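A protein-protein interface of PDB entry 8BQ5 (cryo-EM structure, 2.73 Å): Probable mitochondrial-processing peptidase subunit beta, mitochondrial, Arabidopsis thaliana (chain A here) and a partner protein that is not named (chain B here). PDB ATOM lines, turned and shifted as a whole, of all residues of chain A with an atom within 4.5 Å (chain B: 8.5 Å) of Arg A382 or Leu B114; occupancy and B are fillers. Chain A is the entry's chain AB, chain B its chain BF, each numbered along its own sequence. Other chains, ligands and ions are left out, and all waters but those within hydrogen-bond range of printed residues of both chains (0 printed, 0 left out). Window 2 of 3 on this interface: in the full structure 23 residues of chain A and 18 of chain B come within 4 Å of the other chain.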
ATOM      1  N   ASP A 378      29.463 -15.128 -24.549  1.00  0.00           N
ATOM      2  CA  ASP A 378      28.784 -16.353 -24.142  1.00  0.00           C
ATOM      3  C   ASP A 378      28.171 -16.227 -22.754  1.00  0.00           C
ATOM      4  O   ASP A 378      27.094 -16.779 -22.504  1.00  0.00           O
ATOM      5  CB  ASP A 378      29.753 -17.533 -24.184  1.00  0.00           C
ATOM      6  CG  ASP A 378      29.966 -18.061 -25.586  1.00  0.00           C
ATOM      7  OD1 ASP A 378      29.007 -18.037 -26.386  1.00  0.00           O
ATOM      8  OD2 ASP A 378      31.092 -18.508 -25.889  1.00  0.00           O
ATOM      9  N   LEU A 379      28.842 -15.523 -21.838  1.00  0.00           N
ATOM     10  CA  LEU A 379      28.292 -15.336 -20.500  1.00  0.00           C
ATOM     11  C   LEU A 379      26.991 -14.546 -20.553  1.00  0.00           C
ATOM     12  O   LEU A 379      26.023 -14.872 -19.856  1.00  0.00           O
ATOM     13  CB  LEU A 379      29.315 -14.640 -19.602  1.00  0.00           C
ATOM     14  CG  LEU A 379      28.819 -14.212 -18.220  1.00  0.00           C
ATOM     15  CD1 LEU A 379      28.394 -15.422 -17.406  1.00  0.00           C
ATOM     16  CD2 LEU A 379      29.889 -13.425 -17.487  1.00  0.00           C
ATOM     17  N   THR A 380      26.950 -13.498 -21.377  1.00  0.00           N
ATOM     18  CA  THR A 380      25.709 -12.754 -21.558  1.00  0.00           C
ATOM     19  C   THR A 380      24.640 -13.622 -22.208  1.00  0.00           C
ATOM     20  O   THR A 380      23.461 -13.546 -21.843  1.00  0.00           O
ATOM     21  CB  THR A 380      25.964 -11.500 -22.392  1.00  0.00           C
ATOM     22  OG1 THR A 380      26.920 -10.667 -21.726  1.00  0.00           O
ATOM     23  CG2 THR A 380      24.675 -10.723 -22.585  1.00  0.00           C
ATOM     24  N   GLN A 381      25.034 -14.454 -23.175  1.00  0.00           N
ATOM     25  CA  GLN A 381      24.073 -15.334 -23.831  1.00  0.00           C
ATOM     26  C   GLN A 381      23.454 -16.308 -22.837  1.00  0.00           C
ATOM     27  O   GLN A 381      22.236 -16.512 -22.826  1.00  0.00           O
ATOM     28  CB  GLN A 381      24.751 -16.094 -24.969  1.00  0.00           C
ATOM     29  CG  GLN A 381      24.756 -15.357 -26.288  1.00  0.00           C
ATOM     30  CD  GLN A 381      25.511 -16.110 -27.358  1.00  0.00           C
ATOM     31  OE1 GLN A 381      24.942 -16.946 -28.060  1.00  0.00           O
ATOM     32  NE2 GLN A 381      26.799 -15.824 -27.487  1.00  0.00           N
ATOM     33  N   ARG A 382      24.283 -16.911 -21.983  1.00  0.00           N
ATOM     34  CA  ARG A 382      23.776 -17.866 -21.002  1.00  0.00           C
ATOM     35  C   ARG A 382      22.825 -17.192 -20.022  1.00  0.00           C
ATOM     36  O   ARG A 382      21.802 -17.767 -19.634  1.00  0.00           O
ATOM     37  CB  ARG A 382      24.942 -18.519 -20.259  1.00  0.00           C
ATOM     38  CG  ARG A 382      25.486 -19.764 -20.934  1.00  0.00           C
ATOM     39  CD  ARG A 382      26.753 -20.256 -20.253  1.00  0.00           C
ATOM     40  NE  ARG A 382      27.634 -20.961 -21.176  1.00  0.00           N
ATOM     41  CZ  ARG A 382      27.415 -22.185 -21.639  1.00  0.00           C
ATOM     42  NH1 ARG A 382      26.353 -22.885 -21.274  1.00  0.00           N
ATOM     43  NH2 ARG A 382      28.286 -22.722 -22.488  1.00  0.00           N
ATOM     44  N   VAL A 383      23.153 -15.971 -19.599  1.00  0.00           N
ATOM     45  CA  VAL A 383      22.313 -15.263 -18.638  1.00  0.00           C
ATOM     46  C   VAL A 383      21.000 -14.840 -19.286  1.00  0.00           C
ATOM     47  O   VAL A 383      19.920 -15.003 -18.707  1.00  0.00           O
ATOM     48  CB  VAL A 383      23.072 -14.057 -18.053  1.00  0.00           C
ATOM     49  CG1 VAL A 383      22.133 -13.165 -17.268  1.00  0.00           C
ATOM     50  CG2 VAL A 383      24.215 -14.533 -17.174  1.00  0.00           C
ATOM     51  N   ALA A 384      21.073 -14.297 -20.503  1.00  0.00           N
ATOM     52  CA  ALA A 384      19.873 -13.785 -21.158  1.00  0.00           C
ATOM     53  C   ALA A 384      18.965 -14.903 -21.653  1.00  0.00           C
ATOM     54  O   ALA A 384      17.738 -14.760 -21.619  1.00  0.00           O
ATOM     55  CB  ALA A 384      20.258 -12.868 -22.317  1.00  0.00           C
ATOM     56  N   ILE A 385      19.537 -16.011 -22.127  1.00  0.00           N
ATOM     57  CA  ILE A 385      18.716 -17.097 -22.655  1.00  0.00           C
ATOM     58  C   ILE A 385      17.940 -17.778 -21.535  1.00  0.00           C
ATOM     59  O   ILE A 385      16.748 -18.074 -21.679  1.00  0.00           O
ATOM     60  CB  ILE A 385      19.591 -18.099 -23.430  1.00  0.00           C
ATOM     61  CG1 ILE A 385      19.869 -17.584 -24.843  1.00  0.00           C
ATOM     62  CG2 ILE A 385      18.929 -19.466 -23.487  1.00  0.00           C
ATOM     63  CD1 ILE A 385      21.122 -18.159 -25.460  1.00  0.00           C
ATOM     64  N   ASN A 386      18.596 -18.034 -20.408  1.00  0.00           N
ATOM     65  CA  ASN A 386      17.988 -18.765 -19.306  1.00  0.00           C
ATOM     66  C   ASN A 386      17.389 -17.858 -18.240  1.00  0.00           C
ATOM     67  O   ASN A 386      16.792 -18.365 -17.286  1.00  0.00           O
ATOM     68  CB  ASN A 386      19.020 -19.702 -18.673  1.00  0.00           C
ATOM     69  CG  ASN A 386      19.645 -20.639 -19.685  1.00  0.00           C
ATOM     70  OD1 ASN A 386      19.130 -21.726 -19.941  1.00  0.00           O
ATOM     71  ND2 ASN A 386      20.761 -20.221 -20.267  1.00  0.00           N
ATOM     72  N   ILE A 388      18.669 -15.873 -15.750  1.00  0.00           N
ATOM     73  CA  ILE A 388      19.205 -16.279 -14.460  1.00  0.00           C
ATOM     74  C   ILE A 388      19.832 -15.104 -13.711  1.00  0.00           C
ATOM     75  O   ILE A 388      20.567 -15.308 -12.752  1.00  0.00           O
ATOM     76  CB  ILE A 388      20.206 -17.439 -14.619  1.00  0.00           C
ATOM     77  CG1 ILE A 388      21.262 -17.095 -15.668  1.00  0.00           C
ATOM     78  CG2 ILE A 388      19.480 -18.718 -14.991  1.00  0.00           C
ATOM     79  CD1 ILE A 388      22.547 -17.867 -15.508  1.00  0.00           C
ATOM     80  N   ALA A 422      27.494 -20.459 -14.294  1.00  0.00           N
ATOM     81  CA  ALA A 422      27.697 -19.833 -15.597  1.00  0.00           C
ATOM     82  C   ALA A 422      28.848 -18.839 -15.570  1.00  0.00           C
ATOM     83  O   ALA A 422      29.638 -18.767 -16.518  1.00  0.00           O
ATOM     84  CB  ALA A 422      26.409 -19.149 -16.055  1.00  0.00           C
ATOM     85  N   TYR A 425      32.185 -20.784 -15.254  1.00  0.00           N
ATOM     86  CA  TYR A 425      32.459 -21.537 -16.475  1.00  0.00           C
ATOM     87  C   TYR A 425      33.034 -20.638 -17.560  1.00  0.00           C
ATOM     88  O   TYR A 425      34.040 -20.977 -18.194  1.00  0.00           O
ATOM     89  CB  TYR A 425      31.184 -22.218 -16.972  1.00  0.00           C
ATOM     90  CG  TYR A 425      31.404 -23.103 -18.177  1.00  0.00           C
ATOM     91  CD1 TYR A 425      31.818 -24.419 -18.031  1.00  0.00           C
ATOM     92  CD2 TYR A 425      31.205 -22.618 -19.463  1.00  0.00           C
ATOM     93  CE1 TYR A 425      32.022 -25.227 -19.130  1.00  0.00           C
ATOM     94  CE2 TYR A 425      31.410 -23.418 -20.568  1.00  0.00           C
ATOM     95  CZ  TYR A 425      31.819 -24.722 -20.395  1.00  0.00           C
ATOM     96  OH  TYR A 425      32.021 -25.524 -21.491  1.00  0.00           O
ATOM     97  N   GLU A 426      32.412 -19.481 -17.785  1.00  0.00           N
ATOM     98  CA  GLU A 426      32.840 -18.623 -18.882  1.00  0.00           C
ATOM     99  C   GLU A 426      34.139 -17.896 -18.561  1.00  0.00           C
ATOM    100  O   GLU A 426      34.911 -17.581 -19.472  1.00  0.00           O
ATOM    101  CB  GLU A 426      31.734 -17.626 -19.228  1.00  0.00           C
ATOM    102  CG  GLU A 426      30.499 -18.271 -19.838  1.00  0.00           C
ATOM    103  CD  GLU A 426      30.773 -18.937 -21.177  1.00  0.00           C
ATOM    104  OE1 GLU A 426      31.790 -18.604 -21.820  1.00  0.00           O
ATOM    105  OE2 GLU A 426      29.966 -19.797 -21.587  1.00  0.00           O
ATOM    106  N   GLU B 104      17.233 -20.990 -38.578  1.00  0.00           N
ATOM    107  CA  GLU B 104      17.766 -20.126 -37.529  1.00  0.00           C
ATOM    108  C   GLU B 104      18.799 -20.856 -36.683  1.00  0.00           C
ATOM    109  O   GLU B 104      19.807 -20.266 -36.274  1.00  0.00           O
ATOM    110  CB  GLU B 104      16.627 -19.602 -36.655  1.00  0.00           C
ATOM    111  CG  GLU B 104      16.203 -18.185 -36.987  1.00  0.00           C
ATOM    112  CD  GLU B 104      14.700 -18.006 -36.956  1.00  0.00           C
ATOM    113  OE1 GLU B 104      14.047 -18.605 -36.077  1.00  0.00           O
ATOM    114  OE2 GLU B 104      14.173 -17.264 -37.810  1.00  0.00           O
ATOM    115  N   ARG B 105      18.561 -22.139 -36.401  1.00  0.00           N
ATOM    116  CA  ARG B 105      19.510 -22.921 -35.613  1.00  0.00           C
ATOM    117  C   ARG B 105      20.849 -23.042 -36.326  1.00  0.00           C
ATOM    118  O   ARG B 105      21.911 -22.912 -35.707  1.00  0.00           O
ATOM    119  CB  ARG B 105      18.932 -24.307 -35.331  1.00  0.00           C
ATOM    120  CG  ARG B 105      17.891 -24.343 -34.236  1.00  0.00           C
ATOM    121  CD  ARG B 105      18.497 -24.802 -32.927  1.00  0.00           C
ATOM    122  NE  ARG B 105      18.125 -26.176 -32.612  1.00  0.00           N
ATOM    123  CZ  ARG B 105      18.877 -27.010 -31.907  1.00  0.00           C
ATOM    124  NH1 ARG B 105      20.045 -26.637 -31.409  1.00  0.00           N
ATOM    125  NH2 ARG B 105      18.445 -28.250 -31.693  1.00  0.00           N
ATOM    126  N   GLU B 107      22.080 -21.020 -38.605  1.00  0.00           N
ATOM    127  CA  GLU B 107      22.722 -19.711 -38.669  1.00  0.00           C
ATOM    128  C   GLU B 107      23.430 -19.381 -37.359  1.00  0.00           C
ATOM    129  O   GLU B 107      24.526 -18.810 -37.364  1.00  0.00           O
ATOM    130  CB  GLU B 107      21.684 -18.644 -39.017  1.00  0.00           C
ATOM    131  CG  GLU B 107      22.181 -17.213 -38.928  1.00  0.00           C
ATOM    132  CD  GLU B 107      21.055 -16.202 -39.037  1.00  0.00           C
ATOM    133  OE1 GLU B 107      20.160 -16.211 -38.166  1.00  0.00           O
ATOM    134  OE2 GLU B 107      21.062 -15.402 -39.995  1.00  0.00           O
ATOM    135  N   ARG B 108      22.816 -19.735 -36.227  1.00  0.00           N
ATOM    136  CA  ARG B 108      23.475 -19.554 -34.936  1.00  0.00           C
ATOM    137  C   ARG B 108      24.746 -20.387 -34.846  1.00  0.00           C
ATOM    138  O   ARG B 108      25.782 -19.907 -34.371  1.00  0.00           O
ATOM    139  CB  ARG B 108      22.518 -19.931 -33.806  1.00  0.00           C
ATOM    140  CG  ARG B 108      21.540 -18.848 -33.407  1.00  0.00           C
ATOM    141  CD  ARG B 108      20.801 -19.237 -32.137  1.00  0.00           C
ATOM    142  NE  ARG B 108      21.522 -18.844 -30.934  1.00  0.00           N
ATOM    143  CZ  ARG B 108      21.508 -17.622 -30.421  1.00  0.00           C
ATOM    144  NH1 ARG B 108      20.816 -16.645 -30.982  1.00  0.00           N
ATOM    145  NH2 ARG B 108      22.203 -17.374 -29.315  1.00  0.00           N
ATOM    146  N   GLU B 109      24.683 -21.642 -35.297  1.00  0.00           N
ATOM    147  CA  GLU B 109      25.847 -22.520 -35.239  1.00  0.00           C
ATOM    148  C   GLU B 109      26.968 -22.017 -36.141  1.00  0.00           C
ATOM    149  O   GLU B 109      28.148 -22.098 -35.779  1.00  0.00           O
ATOM    150  CB  GLU B 109      25.437 -23.943 -35.618  1.00  0.00           C
ATOM    151  CG  GLU B 109      26.569 -24.822 -36.123  1.00  0.00           C
ATOM    152  CD  GLU B 109      26.102 -25.842 -37.144  1.00  0.00           C
ATOM    153  OE1 GLU B 109      25.505 -25.435 -38.163  1.00  0.00           O
ATOM    154  OE2 GLU B 109      26.331 -27.049 -36.927  1.00  0.00           O
ATOM    155  N   LEU B 111      27.775 -18.972 -36.924  1.00  0.00           N
ATOM    156  CA  LEU B 111      28.423 -17.788 -36.381  1.00  0.00           C
ATOM    157  C   LEU B 111      29.001 -18.013 -34.988  1.00  0.00           C
ATOM    158  O   LEU B 111      29.514 -17.066 -34.384  1.00  0.00           O
ATOM    159  CB  LEU B 111      27.442 -16.615 -36.360  1.00  0.00           C
ATOM    160  CG  LEU B 111      27.216 -15.949 -37.719  1.00  0.00           C
ATOM    161  CD1 LEU B 111      26.191 -14.837 -37.612  1.00  0.00           C
ATOM    162  CD2 LEU B 111      28.527 -15.418 -38.272  1.00  0.00           C
ATOM    163  N   GLY B 112      28.933 -19.237 -34.469  1.00  0.00           N
ATOM    164  CA  GLY B 112      29.552 -19.545 -33.197  1.00  0.00           C
ATOM    165  C   GLY B 112      28.769 -19.142 -31.970  1.00  0.00           C
ATOM    166  O   GLY B 112      29.372 -18.902 -30.920  1.00  0.00           O
ATOM    167  N   ALA B 113      27.448 -19.059 -32.064  1.00  0.00           N
ATOM    168  CA  ALA B 113      26.623 -18.701 -30.922  1.00  0.00           C
ATOM    169  C   ALA B 113      26.143 -19.947 -30.186  1.00  0.00           C
ATOM    170  O   ALA B 113      26.091 -21.047 -30.740  1.00  0.00           O
ATOM    171  CB  ALA B 113      25.424 -17.863 -31.362  1.00  0.00           C
ATOM    172  N   LEU B 114      25.797 -19.756 -28.916  1.00  0.00           N
ATOM    173  CA  LEU B 114      25.242 -20.838 -28.122  1.00  0.00           C
ATOM    174  C   LEU B 114      23.833 -21.180 -28.604  1.00  0.00           C
ATOM    175  O   LEU B 114      23.107 -20.310 -29.090  1.00  0.00           O
ATOM    176  CB  LEU B 114      25.201 -20.451 -26.647  1.00  0.00           C
ATOM    177  CG  LEU B 114      26.545 -20.284 -25.941  1.00  0.00           C
ATOM    178  CD1 LEU B 114      26.337 -19.765 -24.531  1.00  0.00           C
ATOM    179  CD2 LEU B 114      27.298 -21.602 -25.924  1.00  0.00           C
ATOM    180  N   PRO B 115      23.425 -22.443 -28.485  1.00  0.00           N
ATOM    181  CA  PRO B 115      22.061 -22.810 -28.878  1.00  0.00           C
ATOM    182  C   PRO B 115      21.033 -22.136 -27.984  1.00  0.00           C
ATOM    183  O   PRO B 115      21.277 -21.877 -26.805  1.00  0.00           O
ATOM    184  CB  PRO B 115      22.034 -24.335 -28.706  1.00  0.00           C
ATOM    185  CG  PRO B 115      23.461 -24.754 -28.583  1.00  0.00           C
ATOM    186  CD  PRO B 115      24.190 -23.598 -27.990  1.00  0.00           C
ATOM    187  N   LEU B 116      19.870 -21.847 -28.564  1.00  0.00           N
ATOM    188  CA  LEU B 116      18.777 -21.282 -27.786  1.00  0.00           C
ATOM    189  C   LEU B 116      18.103 -22.308 -26.889  1.00  0.00           C
ATOM    190  O   LEU B 116      17.327 -21.922 -26.009  1.00  0.00           O
ATOM    191  CB  LEU B 116      17.737 -20.650 -28.714  1.00  0.00           C
ATOM    192  CG  LEU B 116      18.119 -19.326 -29.376  1.00  0.00           C
ATOM    193  CD1 LEU B 116      16.971 -18.816 -30.227  1.00  0.00           C
ATOM    194  CD2 LEU B 116      18.522 -18.294 -28.338  1.00  0.00           C
ATOM    195  N   TYR B 117      18.377 -23.594 -27.089  1.00  0.00           N
ATOM    196  CA  TYR B 117      17.774 -24.664 -26.305  1.00  0.00           C
ATOM    197  C   TYR B 117      18.560 -25.941 -26.559  1.00  0.00           C
ATOM    198  O   TYR B 117      19.073 -26.165 -27.660  1.00  0.00           O
ATOM    199  CB  TYR B 117      16.296 -24.858 -26.659  1.00  0.00           C
ATOM    200  CG  TYR B 117      16.023 -24.767 -28.141  1.00  0.00           C
ATOM    201  CD1 TYR B 117      16.211 -25.862 -28.969  1.00  0.00           C
ATOM    202  CD2 TYR B 117      15.591 -23.579 -28.713  1.00  0.00           C
ATOM    203  CE1 TYR B 117      15.967 -25.783 -30.321  1.00  0.00           C
ATOM    204  CE2 TYR B 117      15.351 -23.489 -30.066  1.00  0.00           C
ATOM    205  CZ  TYR B 117      15.539 -24.593 -30.865  1.00  0.00           C
ATOM    206  OH  TYR B 117      15.296 -24.507 -32.215  1.00  0.00           O
ATOM    207  N   GLN B 118      18.686 -26.756 -25.511  1.00  0.00           N
ATOM    208  CA  GLN B 118      19.401 -28.052 -25.621  1.00  0.00           C
ATOM    209  C   GLN B 118      18.520 -29.148 -25.011  1.00  0.00           C
ATOM    210  O   GLN B 118      17.620 -28.813 -24.216  1.00  0.00           O
ATOM    211  CB  GLN B 118      20.743 -27.997 -24.890  1.00  0.00           C
ATOM    212  CG  GLN B 118      21.774 -27.084 -25.529  1.00  0.00           C
ATOM    213  CD  GLN B 118      23.061 -27.080 -24.744  1.00  0.00           C
ATOM    214  OE1 GLN B 118      23.143 -26.524 -23.653  1.00  0.00           O
ATOM    215  NE2 GLN B 118      24.082 -27.710 -25.299  1.00  0.00           N
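The side-chain amide nitrogen of Gln A381 lies within hydrogen-bond range of the side-chain carboxylate of Asp A378, at 3.3 Å. The backbone carbonyl oxygen of Arg A382 sits at hydrogen-bond distance from the side-chain amide nitrogen of Asn A386 (2.7 Å). NE of Arg B108 lies within hydrogen-bond range of O of Leu B114 (2.8 Å). NE of Arg A382 is in salt-bridge range of OE2 of Glu A426 (2.6 Å). N of Ala B113 lies within hydrogen-bond range of O of Arg B108.
The side-chain amide oxygen (OE1) of Gln A381 lies within hydrogen-bond range of the backbone NH (N) of Leu B114, 3.1 Å away. The guanidinium group (NH2) of Arg B108 lies within hydrogen-bond range of the side-chain amide oxygen (OE1) of Gln A381 (3.0 Å).
Printed residues of chain B within 4 Å of Gln A381: Arg B108 (3.0 Å), Ala B113 (3.5 Å) and Leu B114 (3.1 Å). Of the printed residues of chain A, Arg B108 touches Gln A381 (3.0 Å). Leu B114 touches just these residues of chain A: Asp A378 (3.4 Å), Gln A381 (3.1 Å) and Arg A382 (3.7 Å). Of the printed residues of chain A, Pro B115 touches Ile A385 (3.96 Å). The nearest printed residue of chain A that does not touch Leu B114 is Ile A385 (4.7 Å). The nearest printed residue of chain A that does not touch Leu B116 is Asn A386 (6.3 Å).
Of the 13 printed residues of chain B, 5 touch a printed residue of chain A. Hydrophobic or aromatic side chains of chain B that line the printed part of chain A: Ala B113, Leu B114 and Leu B116. Among the printed residues, no Asp or Glu carboxylate lies within 4 Å of a Lys or Arg side-chain nitrogen of the other chain.
Among the printed residues, merely in contact across the chains: Asp A378 with Leu B114 (3.4 Å), Gln A381 with Ala B113 (3.5 Å), Arg A382 with Leu B114 (3.7 Å), Ile A385 with Leu B116 (3.8 Å) and Ile A385 with Pro B115 (3.96 Å).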
